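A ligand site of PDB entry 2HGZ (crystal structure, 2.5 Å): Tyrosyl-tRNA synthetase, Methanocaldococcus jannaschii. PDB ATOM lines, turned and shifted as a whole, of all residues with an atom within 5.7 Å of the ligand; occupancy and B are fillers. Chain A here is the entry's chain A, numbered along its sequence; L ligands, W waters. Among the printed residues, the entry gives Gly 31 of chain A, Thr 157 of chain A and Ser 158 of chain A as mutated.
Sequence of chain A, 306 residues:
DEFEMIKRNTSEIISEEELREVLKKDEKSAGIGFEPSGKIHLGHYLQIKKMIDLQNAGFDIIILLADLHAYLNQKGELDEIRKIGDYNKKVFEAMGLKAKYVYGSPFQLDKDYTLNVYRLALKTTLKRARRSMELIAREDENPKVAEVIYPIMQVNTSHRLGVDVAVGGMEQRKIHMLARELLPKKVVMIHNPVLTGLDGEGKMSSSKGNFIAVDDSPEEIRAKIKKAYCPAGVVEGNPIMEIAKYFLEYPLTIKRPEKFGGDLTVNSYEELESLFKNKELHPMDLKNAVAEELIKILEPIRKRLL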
ATOM      1  N   GLY A  31     -30.646 -12.896 -10.503  1.00  0.00           N
ATOM      2  CA  GLY A  31     -29.410 -13.397 -11.067  1.00  0.00           C
ATOM      3  C   GLY A  31     -28.736 -12.462 -12.054  1.00  0.00           C
ATOM      4  O   GLY A  31     -29.389 -11.650 -12.726  1.00  0.00           O
ATOM      5  N   ILE A  32     -27.425 -12.577 -12.138  1.00  0.00           N
ATOM      6  CA  ILE A  32     -26.655 -11.774 -13.068  1.00  0.00           C
ATOM      7  C   ILE A  32     -25.508 -12.643 -13.545  1.00  0.00           C
ATOM      8  O   ILE A  32     -25.042 -13.512 -12.822  1.00  0.00           O
ATOM      9  CB  ILE A  32     -26.103 -10.492 -12.382  1.00  0.00           C
ATOM     10  CG1 ILE A  32     -25.471  -9.572 -13.430  1.00  0.00           C
ATOM     11  CG2 ILE A  32     -25.073 -10.872 -11.335  1.00  0.00           C
ATOM     12  CD1 ILE A  32     -25.034  -8.235 -12.881  1.00  0.00           C
ATOM     13  N   GLY A  33     -25.074 -12.408 -14.783  1.00  0.00           N
ATOM     14  CA  GLY A  33     -23.975 -13.195 -15.303  1.00  0.00           C
ATOM     15  C   GLY A  33     -22.862 -12.317 -15.804  1.00  0.00           C
ATOM     16  O   GLY A  33     -23.087 -11.205 -16.300  1.00  0.00           O
ATOM     17  N   PHE A  34     -21.637 -12.801 -15.673  1.00  0.00           N
ATOM     18  CA  PHE A  34     -20.474 -12.053 -16.122  1.00  0.00           C
ATOM     19  C   PHE A  34     -19.515 -12.932 -16.873  1.00  0.00           C
ATOM     20  O   PHE A  34     -19.212 -14.050 -16.464  1.00  0.00           O
ATOM     21  CB  PHE A  34     -19.669 -11.473 -14.953  1.00  0.00           C
ATOM     22  CG  PHE A  34     -20.408 -10.465 -14.118  1.00  0.00           C
ATOM     23  CD1 PHE A  34     -20.885 -10.806 -12.859  1.00  0.00           C
ATOM     24  CD2 PHE A  34     -20.541  -9.150 -14.555  1.00  0.00           C
ATOM     25  CE1 PHE A  34     -21.473  -9.852 -12.041  1.00  0.00           C
ATOM     26  CE2 PHE A  34     -21.135  -8.188 -13.737  1.00  0.00           C
ATOM     27  CZ  PHE A  34     -21.596  -8.542 -12.484  1.00  0.00           C
ATOM     28  N   GLU A  35     -19.018 -12.429 -17.997  1.00  0.00           N
ATOM     29  CA  GLU A  35     -18.008 -13.163 -18.711  1.00  0.00           C
ATOM     30  C   GLU A  35     -16.826 -12.858 -17.797  1.00  0.00           C
ATOM     31  O   GLU A  35     -16.596 -11.697 -17.453  1.00  0.00           O
ATOM     32  CB  GLU A  35     -17.763 -12.574 -20.081  1.00  0.00           C
ATOM     33  CG  GLU A  35     -18.809 -12.945 -21.102  1.00  0.00           C
ATOM     34  CD  GLU A  35     -18.453 -12.448 -22.466  1.00  0.00           C
ATOM     35  OE1 GLU A  35     -17.308 -12.719 -22.897  1.00  0.00           O
ATOM     36  OE2 GLU A  35     -19.305 -11.792 -23.102  1.00  0.00           O
ATOM     37  N   ILE A  62     -27.948 -15.240  -7.312  1.00  0.00           N
ATOM     38  CA  ILE A  62     -27.268 -16.206  -8.160  1.00  0.00           C
ATOM     39  C   ILE A  62     -26.329 -15.424  -9.070  1.00  0.00           C
ATOM     40  O   ILE A  62     -26.737 -14.512  -9.789  1.00  0.00           O
ATOM     41  CB  ILE A  62     -28.278 -17.013  -9.007  1.00  0.00           C
ATOM     42  CG1 ILE A  62     -29.186 -17.829  -8.064  1.00  0.00           C
ATOM     43  CG2 ILE A  62     -27.527 -17.932  -9.967  1.00  0.00           C
ATOM     44  CD1 ILE A  62     -30.130 -18.789  -8.754  1.00  0.00           C
ATOM     45  N   LEU A  64     -23.755 -15.920 -12.101  1.00  0.00           N
ATOM     46  CA  LEU A  64     -23.277 -16.848 -13.101  1.00  0.00           C
ATOM     47  C   LEU A  64     -21.915 -16.431 -13.632  1.00  0.00           C
ATOM     48  O   LEU A  64     -21.761 -15.353 -14.220  1.00  0.00           O
ATOM     49  CB  LEU A  64     -24.262 -16.945 -14.262  1.00  0.00           C
ATOM     50  CG  LEU A  64     -23.834 -17.915 -15.374  1.00  0.00           C
ATOM     51  CD1 LEU A  64     -23.875 -19.346 -14.846  1.00  0.00           C
ATOM     52  CD2 LEU A  64     -24.744 -17.749 -16.579  1.00  0.00           C
ATOM     53  N   ALA A  66     -20.062 -16.884 -16.260  1.00  0.00           N
ATOM     54  CA  ALA A  66     -20.298 -17.350 -17.641  1.00  0.00           C
ATOM     55  C   ALA A  66     -19.065 -17.730 -18.443  1.00  0.00           C
ATOM     56  O   ALA A  66     -18.674 -17.021 -19.365  1.00  0.00           O
ATOM     57  CB  ALA A  66     -21.091 -16.278 -18.393  1.00  0.00           C
ATOM     58  N   HIS A  69     -20.039 -18.742 -22.239  1.00  0.00           N
ATOM     59  CA  HIS A  69     -20.355 -17.529 -23.004  1.00  0.00           C
ATOM     60  C   HIS A  69     -19.067 -16.796 -23.346  1.00  0.00           C
ATOM     61  O   HIS A  69     -18.899 -16.311 -24.464  1.00  0.00           O
ATOM     62  CB  HIS A  69     -21.250 -16.569 -22.205  1.00  0.00           C
ATOM     63  CG  HIS A  69     -22.688 -16.960 -22.174  1.00  0.00           C
ATOM     64  ND1 HIS A  69     -23.209 -17.872 -21.275  1.00  0.00           N
ATOM     65  CD2 HIS A  69     -23.742 -16.566 -22.942  1.00  0.00           C
ATOM     66  CE1 HIS A  69     -24.497 -18.030 -21.500  1.00  0.00           C
ATOM     67  NE2 HIS A  69     -24.849 -17.249 -22.507  1.00  0.00           N
ATOM     68  N   GLN A 108     -24.574 -26.115 -19.028  1.00  0.00           N
ATOM     69  CA  GLN A 108     -24.836 -25.598 -20.369  1.00  0.00           C
ATOM     70  C   GLN A 108     -24.410 -26.501 -21.523  1.00  0.00           C
ATOM     71  O   GLN A 108     -24.531 -26.114 -22.686  1.00  0.00           O
ATOM     72  CB  GLN A 108     -24.170 -24.231 -20.537  1.00  0.00           C
ATOM     73  CG  GLN A 108     -24.753 -23.139 -19.666  1.00  0.00           C
ATOM     74  CD  GLN A 108     -23.986 -21.830 -19.798  1.00  0.00           C
ATOM     75  OE1 GLN A 108     -22.759 -21.834 -19.900  1.00  0.00           O
ATOM     76  NE2 GLN A 108     -24.708 -20.716 -19.775  1.00  0.00           N
ATOM     77  N   ILE A 136     -22.179  -6.322 -27.268  1.00  0.00           N
ATOM     78  CA  ILE A 136     -21.506  -7.383 -26.507  1.00  0.00           C
ATOM     79  C   ILE A 136     -20.434  -8.155 -27.281  1.00  0.00           C
ATOM     80  O   ILE A 136     -19.388  -8.479 -26.735  1.00  0.00           O
ATOM     81  CB  ILE A 136     -22.553  -8.386 -25.992  1.00  0.00           C
ATOM     82  CG1 ILE A 136     -23.538  -7.687 -25.070  1.00  0.00           C
ATOM     83  CG2 ILE A 136     -21.870  -9.547 -25.285  1.00  0.00           C
ATOM     84  CD1 ILE A 136     -24.701  -8.555 -24.663  1.00  0.00           C
ATOM     85  N   TYR A 150     -24.281 -17.417 -28.826  1.00  0.00           N
ATOM     86  CA  TYR A 150     -24.185 -16.720 -27.549  1.00  0.00           C
ATOM     87  C   TYR A 150     -25.527 -16.202 -27.014  1.00  0.00           C
ATOM     88  O   TYR A 150     -25.917 -16.524 -25.891  1.00  0.00           O
ATOM     89  CB  TYR A 150     -23.204 -15.571 -27.715  1.00  0.00           C
ATOM     90  CG  TYR A 150     -22.872 -14.814 -26.456  1.00  0.00           C
ATOM     91  CD1 TYR A 150     -21.614 -14.934 -25.868  1.00  0.00           C
ATOM     92  CD2 TYR A 150     -23.791 -13.933 -25.880  1.00  0.00           C
ATOM     93  CE1 TYR A 150     -21.270 -14.176 -24.740  1.00  0.00           C
ATOM     94  CE2 TYR A 150     -23.453 -13.181 -24.758  1.00  0.00           C
ATOM     95  CZ  TYR A 150     -22.202 -13.298 -24.199  1.00  0.00           C
ATOM     96  OH  TYR A 150     -21.865 -12.529 -23.122  1.00  0.00           O
ATOM     97  N   MET A 153     -27.955 -18.835 -26.057  1.00  0.00           N
ATOM     98  CA  MET A 153     -27.408 -19.520 -24.895  1.00  0.00           C
ATOM     99  C   MET A 153     -27.801 -18.718 -23.666  1.00  0.00           C
ATOM    100  O   MET A 153     -28.167 -19.278 -22.636  1.00  0.00           O
ATOM    101  CB  MET A 153     -25.885 -19.592 -24.994  1.00  0.00           C
ATOM    102  CG  MET A 153     -25.352 -20.972 -25.242  1.00  0.00           C
ATOM    103  SD  MET A 153     -25.060 -21.811 -23.690  1.00  0.00           S
ATOM    104  CE  MET A 153     -23.481 -21.048 -23.263  1.00  0.00           C
ATOM    105  N   GLN A 154     -27.709 -17.406 -23.770  1.00  0.00           N
ATOM    106  CA  GLN A 154     -28.082 -16.579 -22.632  1.00  0.00           C
ATOM    107  C   GLN A 154     -29.560 -16.767 -22.328  1.00  0.00           C
ATOM    108  O   GLN A 154     -29.952 -16.833 -21.167  1.00  0.00           O
ATOM    109  CB  GLN A 154     -27.797 -15.114 -22.915  1.00  0.00           C
ATOM    110  CG  GLN A 154     -27.965 -14.265 -21.666  1.00  0.00           C
ATOM    111  CD  GLN A 154     -27.250 -12.941 -21.777  1.00  0.00           C
ATOM    112  OE1 GLN A 154     -26.111 -12.883 -22.248  1.00  0.00           O
ATOM    113  NE2 GLN A 154     -27.898 -11.877 -21.316  1.00  0.00           N
ATOM    114  N   VAL A 155     -30.385 -16.862 -23.365  1.00  0.00           N
ATOM    115  CA  VAL A 155     -31.820 -17.062 -23.175  1.00  0.00           C
ATOM    116  C   VAL A 155     -32.152 -18.415 -22.530  1.00  0.00           C
ATOM    117  O   VAL A 155     -33.046 -18.519 -21.691  1.00  0.00           O
ATOM    118  CB  VAL A 155     -32.577 -16.940 -24.505  1.00  0.00           C
ATOM    119  CG1 VAL A 155     -34.044 -17.317 -24.325  1.00  0.00           C
ATOM    120  CG2 VAL A 155     -32.468 -15.508 -25.036  1.00  0.00           C
ATOM    121  N   THR A 157     -30.245 -20.092 -20.562  1.00  0.00           N
ATOM    122  CA  THR A 157     -29.754 -20.068 -19.200  1.00  0.00           C
ATOM    123  C   THR A 157     -30.786 -19.372 -18.312  1.00  0.00           C
ATOM    124  O   THR A 157     -31.007 -19.781 -17.178  1.00  0.00           O
ATOM    125  CB  THR A 157     -28.387 -19.384 -19.126  1.00  0.00           C
ATOM    126  OG1 THR A 157     -27.407 -20.237 -19.738  1.00  0.00           O
ATOM    127  CG2 THR A 157     -27.978 -19.132 -17.689  1.00  0.00           C
ATOM    128  N   SER A 158     -31.421 -18.318 -18.821  1.00  0.00           N
ATOM    129  CA  SER A 158     -32.440 -17.617 -18.035  1.00  0.00           C
ATOM    130  C   SER A 158     -33.552 -18.614 -17.728  1.00  0.00           C
ATOM    131  O   SER A 158     -34.127 -18.603 -16.640  1.00  0.00           O
ATOM    132  CB  SER A 158     -33.022 -16.440 -18.806  1.00  0.00           C
ATOM    133  OG  SER A 158     -32.044 -15.435 -18.988  1.00  0.00           O
ATOM    134  N   LEU A 161     -31.852 -21.490 -15.127  1.00  0.00           N
ATOM    135  CA  LEU A 161     -31.637 -20.935 -13.805  1.00  0.00           C
ATOM    136  C   LEU A 161     -32.965 -20.596 -13.122  1.00  0.00           C
ATOM    137  O   LEU A 161     -33.073 -20.640 -11.894  1.00  0.00           O
ATOM    138  CB  LEU A 161     -30.776 -19.676 -13.902  1.00  0.00           C
ATOM    139  CG  LEU A 161     -29.306 -19.743 -13.503  1.00  0.00           C
ATOM    140  CD1 LEU A 161     -28.762 -21.143 -13.610  1.00  0.00           C
ATOM    141  CD2 LEU A 161     -28.524 -18.785 -14.383  1.00  0.00           C
ATOM    142  N   VAL A 163     -34.682 -17.750 -12.514  1.00  0.00           N
ATOM    143  CA  VAL A 163     -34.700 -16.682 -11.526  1.00  0.00           C
ATOM    144  C   VAL A 163     -35.930 -15.804 -11.775  1.00  0.00           C
ATOM    145  O   VAL A 163     -36.476 -15.787 -12.869  1.00  0.00           O
ATOM    146  CB  VAL A 163     -33.440 -15.801 -11.608  1.00  0.00           C
ATOM    147  CG1 VAL A 163     -32.213 -16.626 -11.254  1.00  0.00           C
ATOM    148  CG2 VAL A 163     -33.295 -15.203 -13.005  1.00  0.00           C
ATOM    149  N   VAL A 165     -35.881 -12.492 -11.172  1.00  0.00           N
ATOM    150  CA  VAL A 165     -35.305 -11.248 -11.675  1.00  0.00           C
ATOM    151  C   VAL A 165     -33.930 -11.464 -12.282  1.00  0.00           C
ATOM    152  O   VAL A 165     -33.086 -12.194 -11.754  1.00  0.00           O
ATOM    153  CB  VAL A 165     -35.208 -10.195 -10.536  1.00  0.00           C
ATOM    154  CG1 VAL A 165     -34.292  -9.045 -10.938  1.00  0.00           C
ATOM    155  CG2 VAL A 165     -36.609  -9.681 -10.222  1.00  0.00           C
ATOM    156  N   ALA A 166     -33.713 -10.820 -13.424  1.00  0.00           N
ATOM    157  CA  ALA A 166     -32.435 -10.906 -14.102  1.00  0.00           C
ATOM    158  C   ALA A 166     -31.917  -9.486 -14.189  1.00  0.00           C
ATOM    159  O   ALA A 166     -32.628  -8.565 -14.621  1.00  0.00           O
ATOM    160  CB  ALA A 166     -32.611 -11.492 -15.484  1.00  0.00           C
ATOM    161  N   GLU A 171     -26.658  -2.688 -22.059  1.00  0.00           N
ATOM    162  CA  GLU A 171     -26.169  -3.315 -23.274  1.00  0.00           C
ATOM    163  C   GLU A 171     -26.718  -4.720 -23.418  1.00  0.00           C
ATOM    164  O   GLU A 171     -26.624  -5.330 -24.495  1.00  0.00           O
ATOM    165  CB  GLU A 171     -24.628  -3.338 -23.317  1.00  0.00           C
ATOM    166  CG  GLU A 171     -23.953  -4.423 -22.487  1.00  0.00           C
ATOM    167  CD  GLU A 171     -23.931  -4.113 -21.006  1.00  0.00           C
ATOM    168  OE1 GLU A 171     -24.312  -2.977 -20.638  1.00  0.00           O
ATOM    169  OE2 GLU A 171     -23.531  -4.994 -20.206  1.00  0.00           O
ATOM    170  N   GLN A 172     -27.315  -5.230 -22.340  1.00  0.00           N
ATOM    171  CA  GLN A 172     -27.872  -6.581 -22.343  1.00  0.00           C
ATOM    172  C   GLN A 172     -29.345  -6.610 -22.703  1.00  0.00           C
ATOM    173  O   GLN A 172     -29.901  -7.691 -22.915  1.00  0.00           O
ATOM    174  CB  GLN A 172     -27.716  -7.220 -20.955  1.00  0.00           C
ATOM    175  CG  GLN A 172     -26.316  -7.223 -20.379  1.00  0.00           C
ATOM    176  CD  GLN A 172     -25.337  -8.047 -21.198  1.00  0.00           C
ATOM    177  OE1 GLN A 172     -25.666  -9.130 -21.683  1.00  0.00           O
ATOM    178  NE2 GLN A 172     -24.119  -7.547 -21.329  1.00  0.00           N
ATOM    179  N   ILE A 175     -30.703  -8.784 -25.759  1.00  0.00           N
ATOM    180  CA  ILE A 175     -30.706 -10.215 -25.484  1.00  0.00           C
ATOM    181  C   ILE A 175     -31.828 -10.500 -24.474  1.00  0.00           C
ATOM    182  O   ILE A 175     -32.400 -11.584 -24.470  1.00  0.00           O
ATOM    183  CB  ILE A 175     -29.377 -10.706 -24.864  1.00  0.00           C
ATOM    184  CG1 ILE A 175     -28.251 -10.701 -25.908  1.00  0.00           C
ATOM    185  CG2 ILE A 175     -29.554 -12.115 -24.271  1.00  0.00           C
ATOM    186  CD1 ILE A 175     -26.936 -11.227 -25.361  1.00  0.00           C
ATOM    187  N   HIS A 176     -32.138  -9.534 -23.623  1.00  0.00           N
ATOM    188  CA  HIS A 176     -33.188  -9.719 -22.642  1.00  0.00           C
ATOM    189  C   HIS A 176     -34.581  -9.633 -23.285  1.00  0.00           C
ATOM    190  O   HIS A 176     -35.497 -10.342 -22.879  1.00  0.00           O
ATOM    191  CB  HIS A 176     -33.080  -8.684 -21.515  1.00  0.00           C
ATOM    192  CG  HIS A 176     -31.946  -8.940 -20.567  1.00  0.00           C
ATOM    193  ND1 HIS A 176     -31.619  -8.074 -19.551  1.00  0.00           N
ATOM    194  CD2 HIS A 176     -31.060  -9.966 -20.496  1.00  0.00           C
ATOM    195  CE1 HIS A 176     -30.577  -8.559 -18.888  1.00  0.00           C
ATOM    196  NE2 HIS A 176     -30.214  -9.702 -19.448  1.00  0.00           N
HETATM  197  N1  LIG L   1     -23.935 -11.279 -21.565  1.00  0.00           N
HETATM  198  C1  LIG L   1     -21.948 -10.150 -20.535  1.00  0.00           C
HETATM  199  O1  LIG L   1     -21.822  -9.508 -21.652  1.00  0.00           O
HETATM  200  C2  LIG L   1     -23.273 -10.939 -20.289  1.00  0.00           C
HETATM  201  C3  LIG L   1     -22.895 -12.223 -19.621  1.00  0.00           C
HETATM  202  C4  LIG L   1     -24.071 -13.139 -19.291  1.00  0.00           C
HETATM  203  C5  LIG L   1     -24.035 -14.553 -19.553  1.00  0.00           C
HETATM  204  C6  LIG L   1     -25.204 -12.580 -18.698  1.00  0.00           C
HETATM  205  C7  LIG L   1     -25.189 -15.322 -19.193  1.00  0.00           C
HETATM  206  C8  LIG L   1     -26.290 -13.312 -18.355  1.00  0.00           C
HETATM  207  C9  LIG L   1     -26.288 -14.687 -18.601  1.00  0.00           C
HETATM  208  C10 LIG L   1     -27.551 -15.452 -18.189  1.00  0.00           C
HETATM  209  O2  LIG L   1     -28.096 -16.213 -18.951  1.00  0.00           O
HETATM  210  C11 LIG L   1     -28.218 -15.331 -16.859  1.00  0.00           C
HETATM  211  C12 LIG L   1     -27.486 -15.284 -15.689  1.00  0.00           C
HETATM  212  C13 LIG L   1     -29.578 -15.261 -16.902  1.00  0.00           C
HETATM  213  C14 LIG L   1     -28.168 -15.179 -14.464  1.00  0.00           C
HETATM  214  C15 LIG L   1     -30.267 -15.153 -15.706  1.00  0.00           C
HETATM  215  C16 LIG L   1     -29.573 -15.112 -14.476  1.00  0.00           C
HETATM  216  O3  LIG L   1     -21.070 -10.198 -19.538  1.00  0.00           O
HETATM  217  O   HOH W   1     -27.010 -10.589 -16.517  1.00  0.00           O
HETATM  218  O   HOH W   2     -19.394  -8.357 -22.425  1.00  0.00           O
HETATM  219  O   HOH W   3     -29.454 -11.945 -17.843  1.00  0.00           O
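OE1 of Gln 172 is in hydrogen-bond range of N1 of the ligand (2.8 Å). OE1 of Gln 154 lies within hydrogen-bond range of N1 of the ligand, at 2.8 Å. A nitrogen (N1) of the ligand is in hydrogen-bond range of the side-chain hydroxyl of Tyr 150 (2.9 Å). N of Glu 35 is in hydrogen-bond range of O3 of the ligand (3.4 Å).
O of Gln 154 is in hydrogen-bond range of OG of Ser 158, 3.3 Å away. N of Gln 154 is in hydrogen-bond range of NE2 of His 69, 3.1 Å away. OE2 of Glu 35 lies within hydrogen-bond range of OH of Tyr 150 (2.7 Å). OG1 of Thr 157 is in hydrogen-bond range of O of Met 153 (3.1 Å). The side-chain hydroxyl (OG1) of Thr 157 sits at hydrogen-bond distance from the side-chain amide nitrogen (NE2) of Gln 108 (2.7 Å). The backbone carbonyl oxygen (O) of Ile 32 is in hydrogen-bond range of the backbone NH (N) of Leu 64, at 2.8 Å. The backbone NH (N) of Phe 34 is in hydrogen-bond range of the backbone carbonyl oxygen (O) of Leu 64 (2.9 Å). The backbone NH (N) of Ala 66 lies within hydrogen-bond range of the backbone carbonyl oxygen (O) of Phe 34 (3.0 Å).
Gly 31 touches the ligand (C to C14, 3.7 Å). N of Ile 32 touches C14 of the ligand, 3.6 Å away. Gly 33 touches the ligand (O to C3, 3.5 Å). Phe 34 touches the ligand. Leu 64 touches the ligand (CD2 to C7, 3.6 Å). Ala 66 touches the ligand (CB to C5, 3.6 Å). CE1 of His 69 touches C7 of the ligand (3.6 Å). Ile 136 touches the ligand. Thr 157 touches the ligand. OG of Ser 158 touches C13 of the ligand, 3.2 Å away. Leu 161 touches the ligand. Of the 25 residues printed, 15 come within 4 Å of the ligand. The nearest printed residue that does not touch the ligand is Val 163 (4.003 Å).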
